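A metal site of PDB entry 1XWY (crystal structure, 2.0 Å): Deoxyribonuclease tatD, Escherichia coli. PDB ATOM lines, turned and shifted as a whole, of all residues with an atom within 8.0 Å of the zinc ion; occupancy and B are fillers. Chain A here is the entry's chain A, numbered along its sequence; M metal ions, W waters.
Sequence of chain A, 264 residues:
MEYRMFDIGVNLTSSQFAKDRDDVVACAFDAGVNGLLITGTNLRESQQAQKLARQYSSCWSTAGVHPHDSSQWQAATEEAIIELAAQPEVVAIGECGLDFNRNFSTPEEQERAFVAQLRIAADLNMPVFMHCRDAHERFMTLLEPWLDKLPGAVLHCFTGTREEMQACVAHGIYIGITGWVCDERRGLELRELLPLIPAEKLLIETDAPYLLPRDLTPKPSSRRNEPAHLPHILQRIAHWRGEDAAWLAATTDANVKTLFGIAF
The zinc ion is bound by OE1 of Glu 205 (2.0 Å), water W1 (2.1 Å), ND1 of His 156 (2.2 Å) and SG of Cys 157 (2.5 Å). The zinc ion has four donor atoms within binding distance.
The backbone NH of Glu 205 lies within hydrogen-bond range of the backbone carbonyl oxygen of Ile 177 (3.1 Å). A ring nitrogen (NE2) of His 156 sits at hydrogen-bond distance from the side-chain carboxylate of Glu 95. N of His 156 sits close to O of Met 130.
Of the 23 residues printed, 3 come within 4 Å of the zinc ion.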
ATOM      1  N   ASP A   7      -4.914  12.913  19.937  1.00  0.00           N
ATOM      2  CA  ASP A   7      -4.951  13.527  21.279  1.00  0.00           C
ATOM      3  C   ASP A   7      -3.817  12.909  22.120  1.00  0.00           C
ATOM      4  O   ASP A   7      -3.915  11.747  22.537  1.00  0.00           O
ATOM      5  CB  ASP A   7      -6.285  13.227  21.972  1.00  0.00           C
ATOM      6  CG  ASP A   7      -6.512  14.096  23.212  1.00  0.00           C
ATOM      7  OD1 ASP A   7      -5.522  14.553  23.837  1.00  0.00           O
ATOM      8  OD2 ASP A   7      -7.710  14.302  23.563  1.00  0.00           O
ATOM      9  N   ILE A   8      -2.749  13.668  22.358  1.00  0.00           N
ATOM     10  CA  ILE A   8      -1.637  13.097  23.134  1.00  0.00           C
ATOM     11  C   ILE A   8      -1.870  13.062  24.643  1.00  0.00           C
ATOM     12  O   ILE A   8      -1.030  12.547  25.368  1.00  0.00           O
ATOM     13  CB  ILE A   8      -0.277  13.853  22.912  1.00  0.00           C
ATOM     14  CG1 ILE A   8      -0.348  15.256  23.518  1.00  0.00           C
ATOM     15  CG2 ILE A   8       0.048  13.961  21.408  1.00  0.00           C
ATOM     16  CD1 ILE A   8       1.048  15.895  23.822  1.00  0.00           C
ATOM     17  N   GLY A   9      -2.976  13.611  25.117  1.00  0.00           N
ATOM     18  CA  GLY A   9      -3.178  13.622  26.553  1.00  0.00           C
ATOM     19  C   GLY A   9      -4.602  13.341  27.011  1.00  0.00           C
ATOM     20  O   GLY A   9      -5.358  14.266  27.304  1.00  0.00           O
ATOM     21  N   VAL A  10      -4.957  12.059  27.058  1.00  0.00           N
ATOM     22  CA  VAL A  10      -6.298  11.654  27.495  1.00  0.00           C
ATOM     23  C   VAL A  10      -6.159  10.897  28.793  1.00  0.00           C
ATOM     24  O   VAL A  10      -5.480   9.869  28.848  1.00  0.00           O
ATOM     25  CB  VAL A  10      -6.997  10.692  26.506  1.00  0.00           C
ATOM     26  CG1 VAL A  10      -8.485  10.507  26.927  1.00  0.00           C
ATOM     27  CG2 VAL A  10      -6.907  11.214  25.065  1.00  0.00           C
ATOM     28  N   ASN A  11      -6.790  11.405  29.855  1.00  0.00           N
ATOM     29  CA  ASN A  11      -6.748  10.727  31.156  1.00  0.00           C
ATOM     30  C   ASN A  11      -7.947   9.764  31.160  1.00  0.00           C
ATOM     31  O   ASN A  11      -8.889   9.894  31.944  1.00  0.00           O
ATOM     32  CB  ASN A  11      -6.862  11.780  32.271  1.00  0.00           C
ATOM     33  CG  ASN A  11      -5.792  12.869  32.168  1.00  0.00           C
ATOM     34  OD1 ASN A  11      -4.590  12.634  32.408  1.00  0.00           O
ATOM     35  ND2 ASN A  11      -6.215  14.075  31.795  1.00  0.00           N
ATOM     36  N   THR A  39      -2.712   8.560  29.335  1.00  0.00           N
ATOM     37  CA  THR A  39      -1.725   8.884  30.349  1.00  0.00           C
ATOM     38  C   THR A  39      -1.709   7.982  31.586  1.00  0.00           C
ATOM     39  O   THR A  39      -2.740   7.723  32.166  1.00  0.00           O
ATOM     40  CB  THR A  39      -1.910  10.344  30.891  1.00  0.00           C
ATOM     41  OG1 THR A  39      -2.100  11.249  29.807  1.00  0.00           O
ATOM     42  CG2 THR A  39      -0.673  10.793  31.665  1.00  0.00           C
ATOM     43  N   GLU A  95       3.751   9.720  32.622  1.00  0.00           N
ATOM     44  CA  GLU A  95       4.153  11.102  32.939  1.00  0.00           C
ATOM     45  C   GLU A  95       5.217  11.192  34.055  1.00  0.00           C
ATOM     46  O   GLU A  95       5.062  10.595  35.114  1.00  0.00           O
ATOM     47  CB  GLU A  95       2.879  11.878  33.351  1.00  0.00           C
ATOM     48  CG  GLU A  95       3.025  13.405  33.391  1.00  0.00           C
ATOM     49  CD  GLU A  95       1.711  14.086  33.715  1.00  0.00           C
ATOM     50  OE1 GLU A  95       0.718  13.368  33.935  1.00  0.00           O
ATOM     51  OE2 GLU A  95       1.658  15.333  33.757  1.00  0.00           O
ATOM     52  N   PHE A 129       7.383  11.554  28.338  1.00  0.00           N
ATOM     53  CA  PHE A 129       6.165  12.379  28.410  1.00  0.00           C
ATOM     54  C   PHE A 129       6.324  13.097  29.763  1.00  0.00           C
ATOM     55  O   PHE A 129       6.276  12.463  30.826  1.00  0.00           O
ATOM     56  CB  PHE A 129       4.946  11.442  28.397  1.00  0.00           C
ATOM     57  CG  PHE A 129       3.629  12.152  28.262  1.00  0.00           C
ATOM     58  CD1 PHE A 129       3.160  12.533  27.018  1.00  0.00           C
ATOM     59  CD2 PHE A 129       2.818  12.373  29.373  1.00  0.00           C
ATOM     60  CE1 PHE A 129       1.891  13.118  26.884  1.00  0.00           C
ATOM     61  CE2 PHE A 129       1.557  12.962  29.242  1.00  0.00           C
ATOM     62  CZ  PHE A 129       1.099  13.327  27.996  1.00  0.00           C
ATOM     63  N   MET A 130       6.518  14.416  29.721  1.00  0.00           N
ATOM     64  CA  MET A 130       6.826  15.162  30.936  1.00  0.00           C
ATOM     65  C   MET A 130       5.898  16.249  31.448  1.00  0.00           C
ATOM     66  O   MET A 130       5.143  16.874  30.697  1.00  0.00           O
ATOM     67  CB  MET A 130       8.217  15.779  30.794  1.00  0.00           C
ATOM     68  CG  MET A 130       9.259  14.878  30.071  1.00  0.00           C
ATOM     69  SD  MET A 130      10.865  15.673  29.807  1.00  0.00           S
ATOM     70  CE  MET A 130      10.529  16.757  28.464  1.00  0.00           C
ATOM     71  N   VAL A 154       8.457  15.273  25.156  1.00  0.00           N
ATOM     72  CA  VAL A 154       7.427  16.271  25.032  1.00  0.00           C
ATOM     73  C   VAL A 154       7.062  16.791  26.419  1.00  0.00           C
ATOM     74  O   VAL A 154       7.052  16.050  27.400  1.00  0.00           O
ATOM     75  CB  VAL A 154       6.133  15.761  24.320  1.00  0.00           C
ATOM     76  CG1 VAL A 154       5.724  14.408  24.840  1.00  0.00           C
ATOM     77  CG2 VAL A 154       5.000  16.761  24.552  1.00  0.00           C
ATOM     78  N   LEU A 155       6.825  18.075  26.514  1.00  0.00           N
ATOM     79  CA  LEU A 155       6.406  18.684  27.743  1.00  0.00           C
ATOM     80  C   LEU A 155       4.934  19.004  27.441  1.00  0.00           C
ATOM     81  O   LEU A 155       4.640  19.959  26.707  1.00  0.00           O
ATOM     82  CB  LEU A 155       7.217  19.943  28.037  1.00  0.00           C
ATOM     83  CG  LEU A 155       6.983  20.669  29.366  1.00  0.00           C
ATOM     84  CD1 LEU A 155       7.998  21.801  29.569  1.00  0.00           C
ATOM     85  CD2 LEU A 155       5.613  21.293  29.317  1.00  0.00           C
ATOM     86  N   HIS A 156       4.025  18.180  27.963  1.00  0.00           N
ATOM     87  CA  HIS A 156       2.613  18.386  27.701  1.00  0.00           C
ATOM     88  C   HIS A 156       2.004  19.401  28.664  1.00  0.00           C
ATOM     89  O   HIS A 156       2.630  19.804  29.656  1.00  0.00           O
ATOM     90  CB  HIS A 156       1.857  17.054  27.757  1.00  0.00           C
ATOM     91  CG  HIS A 156       1.508  16.609  29.147  1.00  0.00           C
ATOM     92  ND1 HIS A 156       0.214  16.434  29.568  1.00  0.00           N
ATOM     93  CD2 HIS A 156       2.293  16.372  30.228  1.00  0.00           C
ATOM     94  CE1 HIS A 156       0.199  16.123  30.851  1.00  0.00           C
ATOM     95  NE2 HIS A 156       1.456  16.086  31.285  1.00  0.00           N
ATOM     96  N   CYS A 157       0.772  19.812  28.347  1.00  0.00           N
ATOM     97  CA  CYS A 157       0.045  20.793  29.125  1.00  0.00           C
ATOM     98  C   CYS A 157       0.977  21.944  29.455  1.00  0.00           C
ATOM     99  O   CYS A 157       1.075  22.353  30.607  1.00  0.00           O
ATOM    100  CB  CYS A 157      -0.543  20.183  30.406  1.00  0.00           C
ATOM    101  SG  CYS A 157      -2.187  19.424  30.116  1.00  0.00           S
ATOM    102  N   PHE A 158       1.663  22.449  28.447  1.00  0.00           N
ATOM    103  CA  PHE A 158       2.566  23.578  28.653  1.00  0.00           C
ATOM    104  C   PHE A 158       1.776  24.860  28.866  1.00  0.00           C
ATOM    105  O   PHE A 158       0.932  25.233  28.035  1.00  0.00           O
ATOM    106  CB  PHE A 158       3.453  23.780  27.437  1.00  0.00           C
ATOM    107  CG  PHE A 158       4.395  24.960  27.573  1.00  0.00           C
ATOM    108  CD1 PHE A 158       5.570  24.853  28.299  1.00  0.00           C
ATOM    109  CD2 PHE A 158       4.095  26.180  26.974  1.00  0.00           C
ATOM    110  CE1 PHE A 158       6.452  25.942  28.441  1.00  0.00           C
ATOM    111  CE2 PHE A 158       4.952  27.279  27.103  1.00  0.00           C
ATOM    112  CZ  PHE A 158       6.138  27.165  27.840  1.00  0.00           C
ATOM    113  N   GLY A 176       3.134  20.507  24.097  1.00  0.00           N
ATOM    114  CA  GLY A 176       1.740  20.134  24.018  1.00  0.00           C
ATOM    115  C   GLY A 176       0.816  21.275  24.453  1.00  0.00           C
ATOM    116  O   GLY A 176       1.021  21.885  25.495  1.00  0.00           O
ATOM    117  N   ILE A 177      -0.189  21.550  23.634  1.00  0.00           N
ATOM    118  CA  ILE A 177      -1.125  22.625  23.910  1.00  0.00           C
ATOM    119  C   ILE A 177      -2.547  22.054  23.952  1.00  0.00           C
ATOM    120  O   ILE A 177      -2.923  21.254  23.060  1.00  0.00           O
ATOM    121  CB  ILE A 177      -1.060  23.728  22.809  1.00  0.00           C
ATOM    122  CG1 ILE A 177       0.288  24.461  22.882  1.00  0.00           C
ATOM    123  CG2 ILE A 177      -2.174  24.768  23.028  1.00  0.00           C
ATOM    124  CD1 ILE A 177       1.446  23.640  22.425  1.00  0.00           C
ATOM    125  N   THR A 178      -3.308  22.483  24.963  1.00  0.00           N
ATOM    126  CA  THR A 178      -4.688  22.052  25.195  1.00  0.00           C
ATOM    127  C   THR A 178      -5.708  23.187  24.959  1.00  0.00           C
ATOM    128  O   THR A 178      -5.353  24.267  24.470  1.00  0.00           O
ATOM    129  CB  THR A 178      -4.889  21.607  26.668  1.00  0.00           C
ATOM    130  OG1 THR A 178      -4.728  22.756  27.528  1.00  0.00           O
ATOM    131  CG2 THR A 178      -3.864  20.543  27.073  1.00  0.00           C
ATOM    132  N   ILE A 204      -1.088  18.570  20.017  1.00  0.00           N
ATOM    133  CA  ILE A 204      -2.355  19.018  20.587  1.00  0.00           C
ATOM    134  C   ILE A 204      -2.958  17.942  21.493  1.00  0.00           C
ATOM    135  O   ILE A 204      -2.728  16.742  21.306  1.00  0.00           O
ATOM    136  CB  ILE A 204      -3.385  19.377  19.475  1.00  0.00           C
ATOM    137  CG1 ILE A 204      -2.778  20.343  18.455  1.00  0.00           C
ATOM    138  CG2 ILE A 204      -4.632  20.000  20.101  1.00  0.00           C
ATOM    139  CD1 ILE A 204      -2.273  21.636  19.041  1.00  0.00           C
ATOM    140  N   GLU A 205      -3.742  18.375  22.468  1.00  0.00           N
ATOM    141  CA  GLU A 205      -4.333  17.451  23.452  1.00  0.00           C
ATOM    142  C   GLU A 205      -5.544  18.091  24.115  1.00  0.00           C
ATOM    143  O   GLU A 205      -5.731  19.308  24.026  1.00  0.00           O
ATOM    144  CB  GLU A 205      -3.300  17.128  24.512  1.00  0.00           C
ATOM    145  CG  GLU A 205      -2.306  18.278  24.738  1.00  0.00           C
ATOM    146  CD  GLU A 205      -1.494  18.113  25.993  1.00  0.00           C
ATOM    147  OE1 GLU A 205      -1.918  17.314  26.836  1.00  0.00           O
ATOM    148  OE2 GLU A 205      -0.439  18.769  26.149  1.00  0.00           O
ATOM    149  N   THR A 206      -6.383  17.278  24.768  1.00  0.00           N
ATOM    150  CA  THR A 206      -7.530  17.845  25.467  1.00  0.00           C
ATOM    151  C   THR A 206      -7.341  17.900  26.976  1.00  0.00           C
ATOM    152  O   THR A 206      -7.897  18.774  27.630  1.00  0.00           O
ATOM    153  CB  THR A 206      -8.809  17.011  25.267  1.00  0.00           C
ATOM    154  OG1 THR A 206      -8.504  15.646  25.608  1.00  0.00           O
ATOM    155  CG2 THR A 206      -9.303  17.116  23.833  1.00  0.00           C
ATOM    156  N   ASP A 207      -6.544  16.968  27.488  1.00  0.00           N
ATOM    157  CA  ASP A 207      -6.363  16.748  28.931  1.00  0.00           C
ATOM    158  C   ASP A 207      -7.719  16.311  29.495  1.00  0.00           C
ATOM    159  O   ASP A 207      -8.022  16.507  30.674  1.00  0.00           O
ATOM    160  CB  ASP A 207      -5.870  17.992  29.682  1.00  0.00           C
ATOM    161  CG  ASP A 207      -5.389  17.660  31.109  1.00  0.00           C
ATOM    162  OD1 ASP A 207      -4.670  16.638  31.285  1.00  0.00           O
ATOM    163  OD2 ASP A 207      -5.717  18.439  32.062  1.00  0.00           O
ATOM    164  N   ALA A 208      -8.556  15.704  28.649  1.00  0.00           N
ATOM    165  CA  ALA A 208      -9.863  15.235  29.094  1.00  0.00           C
ATOM    166  C   ALA A 208      -9.686  14.310  30.310  1.00  0.00           C
ATOM    167  O   ALA A 208      -8.781  13.478  30.329  1.00  0.00           O
ATOM    168  CB  ALA A 208     -10.587  14.512  27.965  1.00  0.00           C
ATOM    169  N   LEU A 211     -10.275  20.801  31.566  1.00  0.00           N
ATOM    170  CA  LEU A 211     -10.072  21.863  30.596  1.00  0.00           C
ATOM    171  C   LEU A 211     -11.006  21.922  29.414  1.00  0.00           C
ATOM    172  O   LEU A 211     -10.555  22.062  28.270  1.00  0.00           O
ATOM    173  CB  LEU A 211      -8.623  21.783  30.082  1.00  0.00           C
ATOM    174  CG  LEU A 211      -7.561  21.985  31.171  1.00  0.00           C
ATOM    175  CD1 LEU A 211      -6.150  21.956  30.567  1.00  0.00           C
ATOM    176  CD2 LEU A 211      -7.839  23.340  31.881  1.00  0.00           C
HETATM  177 ZN    ZN M   1      -1.582  17.423  28.794  1.00  0.00          ZN
HETATM  178  O   HOH W   1      -2.999  15.968  29.377  1.00  0.00           O
